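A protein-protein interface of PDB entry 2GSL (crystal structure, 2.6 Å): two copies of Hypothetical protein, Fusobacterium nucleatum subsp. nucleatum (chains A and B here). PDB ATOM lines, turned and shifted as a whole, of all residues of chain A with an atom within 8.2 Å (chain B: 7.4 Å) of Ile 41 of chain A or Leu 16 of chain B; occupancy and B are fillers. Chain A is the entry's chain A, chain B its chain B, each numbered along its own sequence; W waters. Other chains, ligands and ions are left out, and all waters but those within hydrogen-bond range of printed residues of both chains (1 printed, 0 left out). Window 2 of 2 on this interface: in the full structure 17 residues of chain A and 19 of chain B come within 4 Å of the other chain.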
ATOM      1  N   ARG A  31      -7.976 -19.973 -10.453  1.00  0.00           N
ATOM      2  CA  ARG A  31      -9.198 -20.730 -10.641  1.00  0.00           C
ATOM      3  C   ARG A  31      -8.889 -22.218 -10.720  1.00  0.00           C
ATOM      4  O   ARG A  31      -9.623 -23.044 -10.161  1.00  0.00           O
ATOM      5  CB  ARG A  31      -9.916 -20.277 -11.892  1.00  0.00           C
ATOM      6  CG  ARG A  31     -10.309 -18.829 -11.832  1.00  0.00           C
ATOM      7  CD  ARG A  31     -11.241 -18.546 -12.958  1.00  0.00           C
ATOM      8  NE  ARG A  31     -11.677 -17.165 -12.995  1.00  0.00           N
ATOM      9  CZ  ARG A  31     -12.500 -16.683 -13.921  1.00  0.00           C
ATOM     10  NH1 ARG A  31     -12.963 -17.491 -14.871  1.00  0.00           N
ATOM     11  NH2 ARG A  31     -12.853 -15.398 -13.914  1.00  0.00           N
ATOM     12  N   LEU A  35     -10.576 -24.906  -8.464  1.00  0.00           N
ATOM     13  CA  LEU A  35     -11.571 -25.656  -9.210  1.00  0.00           C
ATOM     14  C   LEU A  35     -11.376 -27.157  -9.051  1.00  0.00           C
ATOM     15  O   LEU A  35     -11.888 -27.948  -9.845  1.00  0.00           O
ATOM     16  CB  LEU A  35     -11.477 -25.287 -10.686  1.00  0.00           C
ATOM     17  CG  LEU A  35     -12.671 -25.621 -11.585  1.00  0.00           C
ATOM     18  CD1 LEU A  35     -13.935 -24.924 -11.080  1.00  0.00           C
ATOM     19  CD2 LEU A  35     -12.358 -25.175 -13.004  1.00  0.00           C
ATOM     20  N   GLY A  38     -14.353 -28.880  -5.439  1.00  0.00           N
ATOM     21  CA  GLY A  38     -15.756 -29.238  -5.499  1.00  0.00           C
ATOM     22  C   GLY A  38     -16.683 -28.160  -4.962  1.00  0.00           C
ATOM     23  O   GLY A  38     -17.889 -28.372  -4.827  1.00  0.00           O
ATOM     24  N   TYR A  39     -16.132 -26.996  -4.653  1.00  0.00           N
ATOM     25  CA  TYR A  39     -16.942 -25.906  -4.143  1.00  0.00           C
ATOM     26  C   TYR A  39     -18.031 -25.584  -5.156  1.00  0.00           C
ATOM     27  O   TYR A  39     -17.974 -26.033  -6.306  1.00  0.00           O
ATOM     28  CB  TYR A  39     -16.077 -24.666  -3.910  1.00  0.00           C
ATOM     29  CG  TYR A  39     -15.012 -24.848  -2.860  1.00  0.00           C
ATOM     30  CD1 TYR A  39     -13.688 -24.491  -3.113  1.00  0.00           C
ATOM     31  CD2 TYR A  39     -15.326 -25.369  -1.611  1.00  0.00           C
ATOM     32  CE1 TYR A  39     -12.703 -24.654  -2.137  1.00  0.00           C
ATOM     33  CE2 TYR A  39     -14.356 -25.536  -0.632  1.00  0.00           C
ATOM     34  CZ  TYR A  39     -13.052 -25.181  -0.892  1.00  0.00           C
ATOM     35  OH  TYR A  39     -12.094 -25.351   0.085  1.00  0.00           O
ATOM     36  N   ASN A  40     -19.037 -24.831  -4.713  1.00  0.00           N
ATOM     37  CA  ASN A  40     -20.135 -24.399  -5.575  1.00  0.00           C
ATOM     38  C   ASN A  40     -19.729 -23.032  -6.100  1.00  0.00           C
ATOM     39  O   ASN A  40     -18.846 -22.385  -5.540  1.00  0.00           O
ATOM     40  CB  ASN A  40     -21.437 -24.289  -4.782  1.00  0.00           C
ATOM     41  CG  ASN A  40     -21.241 -23.629  -3.435  1.00  0.00           C
ATOM     42  OD1 ASN A  40     -20.758 -22.492  -3.340  1.00  0.00           O
ATOM     43  ND2 ASN A  40     -21.617 -24.338  -2.379  1.00  0.00           N
ATOM     44  N   ILE A  41     -20.380 -22.581  -7.161  1.00  0.00           N
ATOM     45  CA  ILE A  41     -20.012 -21.304  -7.757  1.00  0.00           C
ATOM     46  C   ILE A  41     -19.797 -20.165  -6.768  1.00  0.00           C
ATOM     47  O   ILE A  41     -18.704 -19.594  -6.705  1.00  0.00           O
ATOM     48  CB  ILE A  41     -21.027 -20.880  -8.823  1.00  0.00           C
ATOM     49  CG1 ILE A  41     -21.185 -22.013  -9.845  1.00  0.00           C
ATOM     50  CG2 ILE A  41     -20.544 -19.623  -9.521  1.00  0.00           C
ATOM     51  CD1 ILE A  41     -19.858 -22.483 -10.451  1.00  0.00           C
ATOM     52  N   PRO A  42     -20.822 -19.827  -5.972  1.00  0.00           N
ATOM     53  CA  PRO A  42     -20.669 -18.737  -5.005  1.00  0.00           C
ATOM     54  C   PRO A  42     -19.410 -18.872  -4.156  1.00  0.00           C
ATOM     55  O   PRO A  42     -18.637 -17.928  -4.028  1.00  0.00           O
ATOM     56  CB  PRO A  42     -21.956 -18.818  -4.190  1.00  0.00           C
ATOM     57  CG  PRO A  42     -22.360 -20.260  -4.325  1.00  0.00           C
ATOM     58  CD  PRO A  42     -22.096 -20.535  -5.766  1.00  0.00           C
ATOM     59  N   THR A  43     -19.190 -20.052  -3.592  1.00  0.00           N
ATOM     60  CA  THR A  43     -18.011 -20.288  -2.759  1.00  0.00           C
ATOM     61  C   THR A  43     -16.714 -20.223  -3.565  1.00  0.00           C
ATOM     62  O   THR A  43     -15.756 -19.558  -3.173  1.00  0.00           O
ATOM     63  CB  THR A  43     -18.103 -21.654  -2.093  1.00  0.00           C
ATOM     64  OG1 THR A  43     -19.353 -21.747  -1.399  1.00  0.00           O
ATOM     65  CG2 THR A  43     -16.962 -21.849  -1.117  1.00  0.00           C
ATOM     66  N   LEU A  44     -16.690 -20.946  -4.681  1.00  0.00           N
ATOM     67  CA  LEU A  44     -15.542 -20.972  -5.577  1.00  0.00           C
ATOM     68  C   LEU A  44     -15.087 -19.548  -5.899  1.00  0.00           C
ATOM     69  O   LEU A  44     -13.922 -19.201  -5.714  1.00  0.00           O
ATOM     70  CB  LEU A  44     -15.932 -21.677  -6.871  1.00  0.00           C
ATOM     71  CG  LEU A  44     -14.886 -21.652  -7.982  1.00  0.00           C
ATOM     72  CD1 LEU A  44     -13.631 -22.382  -7.527  1.00  0.00           C
ATOM     73  CD2 LEU A  44     -15.463 -22.309  -9.216  1.00  0.00           C
ATOM     74  N   ASN A  45     -16.027 -18.741  -6.385  1.00  0.00           N
ATOM     75  CA  ASN A  45     -15.775 -17.355  -6.743  1.00  0.00           C
ATOM     76  C   ASN A  45     -15.205 -16.576  -5.561  1.00  0.00           C
ATOM     77  O   ASN A  45     -14.267 -15.793  -5.716  1.00  0.00           O
ATOM     78  CB  ASN A  45     -17.073 -16.703  -7.235  1.00  0.00           C
ATOM     79  CG  ASN A  45     -17.525 -17.238  -8.596  1.00  0.00           C
ATOM     80  OD1 ASN A  45     -17.632 -18.449  -8.802  1.00  0.00           O
ATOM     81  ND2 ASN A  45     -17.795 -16.328  -9.528  1.00  0.00           N
ATOM     82  N   LYS A  46     -15.771 -16.800  -4.380  1.00  0.00           N
ATOM     83  CA  LYS A  46     -15.313 -16.131  -3.167  1.00  0.00           C
ATOM     84  C   LYS A  46     -13.833 -16.388  -2.877  1.00  0.00           C
ATOM     85  O   LYS A  46     -13.102 -15.458  -2.529  1.00  0.00           O
ATOM     86  CB  LYS A  46     -16.154 -16.586  -1.973  1.00  0.00           C
ATOM     87  CG  LYS A  46     -15.696 -16.024  -0.637  1.00  0.00           C
ATOM     88  CD  LYS A  46     -16.560 -16.525   0.507  1.00  0.00           C
ATOM     89  CE  LYS A  46     -16.430 -18.021   0.701  1.00  0.00           C
ATOM     90  NZ  LYS A  46     -17.440 -18.497   1.695  1.00  0.00           N
ATOM     91  N   TYR A  47     -13.398 -17.641  -3.007  1.00  0.00           N
ATOM     92  CA  TYR A  47     -11.991 -17.999  -2.763  1.00  0.00           C
ATOM     93  C   TYR A  47     -11.056 -17.442  -3.840  1.00  0.00           C
ATOM     94  O   TYR A  47      -9.890 -17.138  -3.569  1.00  0.00           O
ATOM     95  CB  TYR A  47     -11.798 -19.525  -2.705  1.00  0.00           C
ATOM     96  CG  TYR A  47     -12.261 -20.172  -1.421  1.00  0.00           C
ATOM     97  CD1 TYR A  47     -13.595 -20.106  -1.032  1.00  0.00           C
ATOM     98  CD2 TYR A  47     -11.368 -20.858  -0.595  1.00  0.00           C
ATOM     99  CE1 TYR A  47     -14.036 -20.702   0.144  1.00  0.00           C
ATOM    100  CE2 TYR A  47     -11.800 -21.462   0.588  1.00  0.00           C
ATOM    101  CZ  TYR A  47     -13.142 -21.377   0.950  1.00  0.00           C
ATOM    102  OH  TYR A  47     -13.605 -21.959   2.113  1.00  0.00           O
ATOM    103  N   VAL A  48     -11.574 -17.330  -5.062  1.00  0.00           N
ATOM    104  CA  VAL A  48     -10.798 -16.817  -6.177  1.00  0.00           C
ATOM    105  C   VAL A  48     -10.528 -15.330  -5.992  1.00  0.00           C
ATOM    106  O   VAL A  48      -9.376 -14.890  -6.069  1.00  0.00           O
ATOM    107  CB  VAL A  48     -11.529 -17.031  -7.509  1.00  0.00           C
ATOM    108  CG1 VAL A  48     -10.733 -16.413  -8.639  1.00  0.00           C
ATOM    109  CG2 VAL A  48     -11.726 -18.520  -7.756  1.00  0.00           C
ATOM    110  N   TYR B  13     -16.275 -32.795 -12.639  1.00  0.00           N
ATOM    111  CA  TYR B  13     -16.482 -31.476 -13.226  1.00  0.00           C
ATOM    112  C   TYR B  13     -17.839 -31.267 -13.877  1.00  0.00           C
ATOM    113  O   TYR B  13     -18.265 -32.048 -14.725  1.00  0.00           O
ATOM    114  CB  TYR B  13     -15.380 -31.193 -14.240  1.00  0.00           C
ATOM    115  CG  TYR B  13     -14.036 -31.016 -13.596  1.00  0.00           C
ATOM    116  CD1 TYR B  13     -13.041 -31.981 -13.726  1.00  0.00           C
ATOM    117  CD2 TYR B  13     -13.757 -29.882 -12.854  1.00  0.00           C
ATOM    118  CE1 TYR B  13     -11.795 -31.813 -13.130  1.00  0.00           C
ATOM    119  CE2 TYR B  13     -12.520 -29.705 -12.259  1.00  0.00           C
ATOM    120  CZ  TYR B  13     -11.541 -30.672 -12.401  1.00  0.00           C
ATOM    121  OH  TYR B  13     -10.307 -30.466 -11.818  1.00  0.00           O
ATOM    122  N   SER B  14     -18.522 -30.199 -13.483  1.00  0.00           N
ATOM    123  CA  SER B  14     -19.830 -29.908 -14.047  1.00  0.00           C
ATOM    124  C   SER B  14     -19.717 -28.900 -15.172  1.00  0.00           C
ATOM    125  O   SER B  14     -18.636 -28.389 -15.463  1.00  0.00           O
ATOM    126  CB  SER B  14     -20.762 -29.365 -12.963  1.00  0.00           C
ATOM    127  OG  SER B  14     -20.204 -28.222 -12.338  1.00  0.00           O
ATOM    128  N   GLY B  15     -20.848 -28.611 -15.798  1.00  0.00           N
ATOM    129  CA  GLY B  15     -20.854 -27.661 -16.892  1.00  0.00           C
ATOM    130  C   GLY B  15     -20.258 -26.330 -16.500  1.00  0.00           C
ATOM    131  O   GLY B  15     -19.313 -25.852 -17.127  1.00  0.00           O
ATOM    132  N   LEU B  16     -20.813 -25.734 -15.455  1.00  0.00           N
ATOM    133  CA  LEU B  16     -20.337 -24.454 -14.992  1.00  0.00           C
ATOM    134  C   LEU B  16     -18.896 -24.493 -14.518  1.00  0.00           C
ATOM    135  O   LEU B  16     -18.146 -23.556 -14.756  1.00  0.00           O
ATOM    136  CB  LEU B  16     -21.240 -23.922 -13.877  1.00  0.00           C
ATOM    137  CG  LEU B  16     -22.529 -23.286 -14.383  1.00  0.00           C
ATOM    138  CD1 LEU B  16     -23.389 -24.369 -14.988  1.00  0.00           C
ATOM    139  CD2 LEU B  16     -23.265 -22.569 -13.247  1.00  0.00           C
ATOM    140  N   GLU B  17     -18.497 -25.561 -13.844  1.00  0.00           N
ATOM    141  CA  GLU B  17     -17.119 -25.627 -13.373  1.00  0.00           C
ATOM    142  C   GLU B  17     -16.163 -25.678 -14.560  1.00  0.00           C
ATOM    143  O   GLU B  17     -15.070 -25.114 -14.511  1.00  0.00           O
ATOM    144  CB  GLU B  17     -16.886 -26.853 -12.482  1.00  0.00           C
ATOM    145  CG  GLU B  17     -17.427 -26.734 -11.051  1.00  0.00           C
ATOM    146  CD  GLU B  17     -17.359 -28.052 -10.276  1.00  0.00           C
ATOM    147  OE1 GLU B  17     -18.149 -28.970 -10.602  1.00  0.00           O
ATOM    148  OE2 GLU B  17     -16.514 -28.175  -9.354  1.00  0.00           O
ATOM    149  N   LEU B  18     -16.571 -26.350 -15.626  1.00  0.00           N
ATOM    150  CA  LEU B  18     -15.712 -26.447 -16.793  1.00  0.00           C
ATOM    151  C   LEU B  18     -15.665 -25.096 -17.508  1.00  0.00           C
ATOM    152  O   LEU B  18     -14.623 -24.678 -18.019  1.00  0.00           O
ATOM    153  CB  LEU B  18     -16.218 -27.551 -17.739  1.00  0.00           C
ATOM    154  CG  LEU B  18     -16.084 -29.001 -17.248  1.00  0.00           C
ATOM    155  CD1 LEU B  18     -16.775 -29.957 -18.206  1.00  0.00           C
ATOM    156  CD2 LEU B  18     -14.616 -29.352 -17.103  1.00  0.00           C
ATOM    157  N   ALA B  19     -16.799 -24.410 -17.523  1.00  0.00           N
ATOM    158  CA  ALA B  19     -16.901 -23.115 -18.178  1.00  0.00           C
ATOM    159  C   ALA B  19     -16.057 -22.088 -17.429  1.00  0.00           C
ATOM    160  O   ALA B  19     -15.435 -21.219 -18.038  1.00  0.00           O
ATOM    161  CB  ALA B  19     -18.353 -22.674 -18.219  1.00  0.00           C
ATOM    162  N   PHE B  20     -16.045 -22.195 -16.103  1.00  0.00           N
ATOM    163  CA  PHE B  20     -15.281 -21.292 -15.252  1.00  0.00           C
ATOM    164  C   PHE B  20     -13.808 -21.331 -15.698  1.00  0.00           C
ATOM    165  O   PHE B  20     -13.175 -20.296 -15.924  1.00  0.00           O
ATOM    166  CB  PHE B  20     -15.436 -21.732 -13.782  1.00  0.00           C
ATOM    167  CG  PHE B  20     -14.910 -20.734 -12.780  1.00  0.00           C
ATOM    168  CD1 PHE B  20     -15.390 -19.428 -12.750  1.00  0.00           C
ATOM    169  CD2 PHE B  20     -13.929 -21.103 -11.868  1.00  0.00           C
ATOM    170  CE1 PHE B  20     -14.903 -18.508 -11.827  1.00  0.00           C
ATOM    171  CE2 PHE B  20     -13.434 -20.194 -10.941  1.00  0.00           C
ATOM    172  CZ  PHE B  20     -13.926 -18.891 -10.924  1.00  0.00           C
ATOM    173  N   LEU B  21     -13.264 -22.528 -15.836  1.00  0.00           N
ATOM    174  CA  LEU B  21     -11.885 -22.660 -16.261  1.00  0.00           C
ATOM    175  C   LEU B  21     -11.704 -22.185 -17.718  1.00  0.00           C
ATOM    176  O   LEU B  21     -10.810 -21.389 -18.011  1.00  0.00           O
ATOM    177  CB  LEU B  21     -11.456 -24.109 -16.106  1.00  0.00           C
ATOM    178  CG  LEU B  21     -10.001 -24.410 -16.415  1.00  0.00           C
ATOM    179  CD1 LEU B  21      -9.080 -23.597 -15.526  1.00  0.00           C
ATOM    180  CD2 LEU B  21      -9.779 -25.903 -16.203  1.00  0.00           C
ATOM    181  N   GLY B  22     -12.576 -22.650 -18.612  1.00  0.00           N
ATOM    182  CA  GLY B  22     -12.491 -22.273 -20.014  1.00  0.00           C
ATOM    183  C   GLY B  22     -12.519 -20.783 -20.317  1.00  0.00           C
ATOM    184  O   GLY B  22     -11.875 -20.314 -21.270  1.00  0.00           O
ATOM    185  N   ARG B  78     -24.593 -30.938 -23.117  1.00  0.00           N
ATOM    186  CA  ARG B  78     -25.190 -30.696 -21.814  1.00  0.00           C
ATOM    187  C   ARG B  78     -24.979 -29.263 -21.350  1.00  0.00           C
ATOM    188  O   ARG B  78     -25.793 -28.722 -20.601  1.00  0.00           O
ATOM    189  CB  ARG B  78     -24.650 -31.696 -20.780  1.00  0.00           C
ATOM    190  CG  ARG B  78     -23.151 -31.659 -20.503  1.00  0.00           C
ATOM    191  CD  ARG B  78     -22.712 -33.003 -19.908  1.00  0.00           C
ATOM    192  NE  ARG B  78     -21.399 -32.982 -19.267  1.00  0.00           N
ATOM    193  CZ  ARG B  78     -21.122 -32.332 -18.139  1.00  0.00           C
ATOM    194  NH1 ARG B  78     -22.065 -31.632 -17.519  1.00  0.00           N
ATOM    195  NH2 ARG B  78     -19.903 -32.401 -17.618  1.00  0.00           N
ATOM    196  N   ALA B  79     -23.895 -28.644 -21.816  1.00  0.00           N
ATOM    197  CA  ALA B  79     -23.585 -27.263 -21.450  1.00  0.00           C
ATOM    198  C   ALA B  79     -24.688 -26.291 -21.890  1.00  0.00           C
ATOM    199  O   ALA B  79     -24.846 -25.223 -21.301  1.00  0.00           O
ATOM    200  CB  ALA B  79     -22.243 -26.852 -22.050  1.00  0.00           C
ATOM    201  N   ASN B  81     -27.698 -26.137 -21.278  1.00  0.00           N
ATOM    202  CA  ASN B  81     -28.830 -26.386 -20.379  1.00  0.00           C
ATOM    203  C   ASN B  81     -28.498 -25.941 -18.967  1.00  0.00           C
ATOM    204  O   ASN B  81     -27.442 -26.291 -18.443  1.00  0.00           O
ATOM    205  CB  ASN B  81     -29.170 -27.870 -20.358  1.00  0.00           C
ATOM    206  CG  ASN B  81     -29.750 -28.345 -21.667  1.00  0.00           C
ATOM    207  OD1 ASN B  81     -30.868 -27.969 -22.032  1.00  0.00           O
ATOM    208  ND2 ASN B  81     -28.991 -29.171 -22.394  1.00  0.00           N
ATOM    209  N   THR B 100     -21.238 -20.827 -23.144  1.00  0.00           N
ATOM    210  CA  THR B 100     -20.843 -21.622 -21.986  1.00  0.00           C
ATOM    211  C   THR B 100     -20.300 -22.948 -22.492  1.00  0.00           C
ATOM    212  O   THR B 100     -19.304 -23.475 -21.988  1.00  0.00           O
ATOM    213  CB  THR B 100     -22.056 -21.879 -21.089  1.00  0.00           C
ATOM    214  OG1 THR B 100     -22.700 -20.630 -20.816  1.00  0.00           O
ATOM    215  CG2 THR B 100     -21.635 -22.524 -19.781  1.00  0.00           C
ATOM    216  N   ALA B 104     -16.808 -24.277 -21.633  1.00  0.00           N
ATOM    217  CA  ALA B 104     -16.821 -25.568 -20.973  1.00  0.00           C
ATOM    218  C   ALA B 104     -15.942 -26.550 -21.749  1.00  0.00           C
ATOM    219  O   ALA B 104     -15.147 -27.287 -21.162  1.00  0.00           O
ATOM    220  CB  ALA B 104     -18.254 -26.078 -20.878  1.00  0.00           C
HETATM  221  O   HOH W   1     -15.184 -25.849  -7.725  1.00  0.00           O
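The guanidinium group of Arg 31 of chain A is in hydrogen-bond range of the backbone carbonyl oxygen of Phe 20 of chain B.
O of Ile 41 of chain A lies close to OD1 of Asn 45 of chain A.
The backbone carbonyl oxygen (O) of Tyr 13 of chain B lies within hydrogen-bond range of the guanidinium group (NH2) of Arg 78 of chain B, at 3.3 Å.
OE1 of Glu 17 of chain B lies within hydrogen-bond range of OG of Ser 14 of chain B (2.8 Å).
Tyr 13 of chain B touches Leu 35 of chain A (CE2 to O, 3.1 Å).
Leu 35 of chain A touches Glu 17 of chain B (CD2 to O, 3.1 Å).
CD2 of Phe 20 of chain B touches CD1 of Leu 35 of chain A, at 3.9 Å.
CD2 of Leu 35 of chain A touches CB of Leu 21 of chain B, 3.4 Å away.
CD1 of Ile 41 of chain A touches CB of Leu 16 of chain B, at 3.96 Å.
Phe 20 of chain B touches Leu 44 of chain A (CD2 to CD2, 3.3 Å).
CG2 of Val 48 of chain A touches CZ of Phe 20 of chain B, at 3.9 Å.
Of the printed residues of chain B, Ile 41 of chain A touches Leu 16.
Of the printed residues of chain A, Leu 16 of chain B touches Ile 41 (3.96 Å).
Of the printed residues of chain B, Leu 35 of chain A touches Tyr 13, Glu 17, Phe 20 and Leu 21.
Of the printed residues of chain A, Leu 21 of chain B touches Leu 35 (3.4 Å).
The nearest residue of chain B that does not touch Ile 41 of chain A is Glu 17 of chain B (4.8 Å).
The nearest residue of chain A that does not touch Leu 16 of chain B is Leu 35 of chain A (5.8 Å).
The nearest printed residue of chain B that does not touch Leu 44 of chain A is Glu 17 of chain B (5.2 Å).
Of the 15 printed residues of chain B, 5 touch a printed residue of chain A.
Hydrophobic or aromatic side chains of chain A that line the printed part of chain B: Leu 35, Ile 41, Leu 44 and Val 48.
Among the printed residues, no Asp or Glu carboxylate lies within 4 Å of a Lys or Arg side-chain nitrogen of the other chain.
No position is printed for both chains.
Of the 8 pairs that touch across the chains among the printed residues, none has its exchanged pair printed and touching as well.
Water W1 bridges the backbone carbonyl oxygen (O) of Tyr 39 of chain A (3.1 Å) and the side-chain carboxylate (OE2) of Glu 17 of chain B (3.1 Å).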
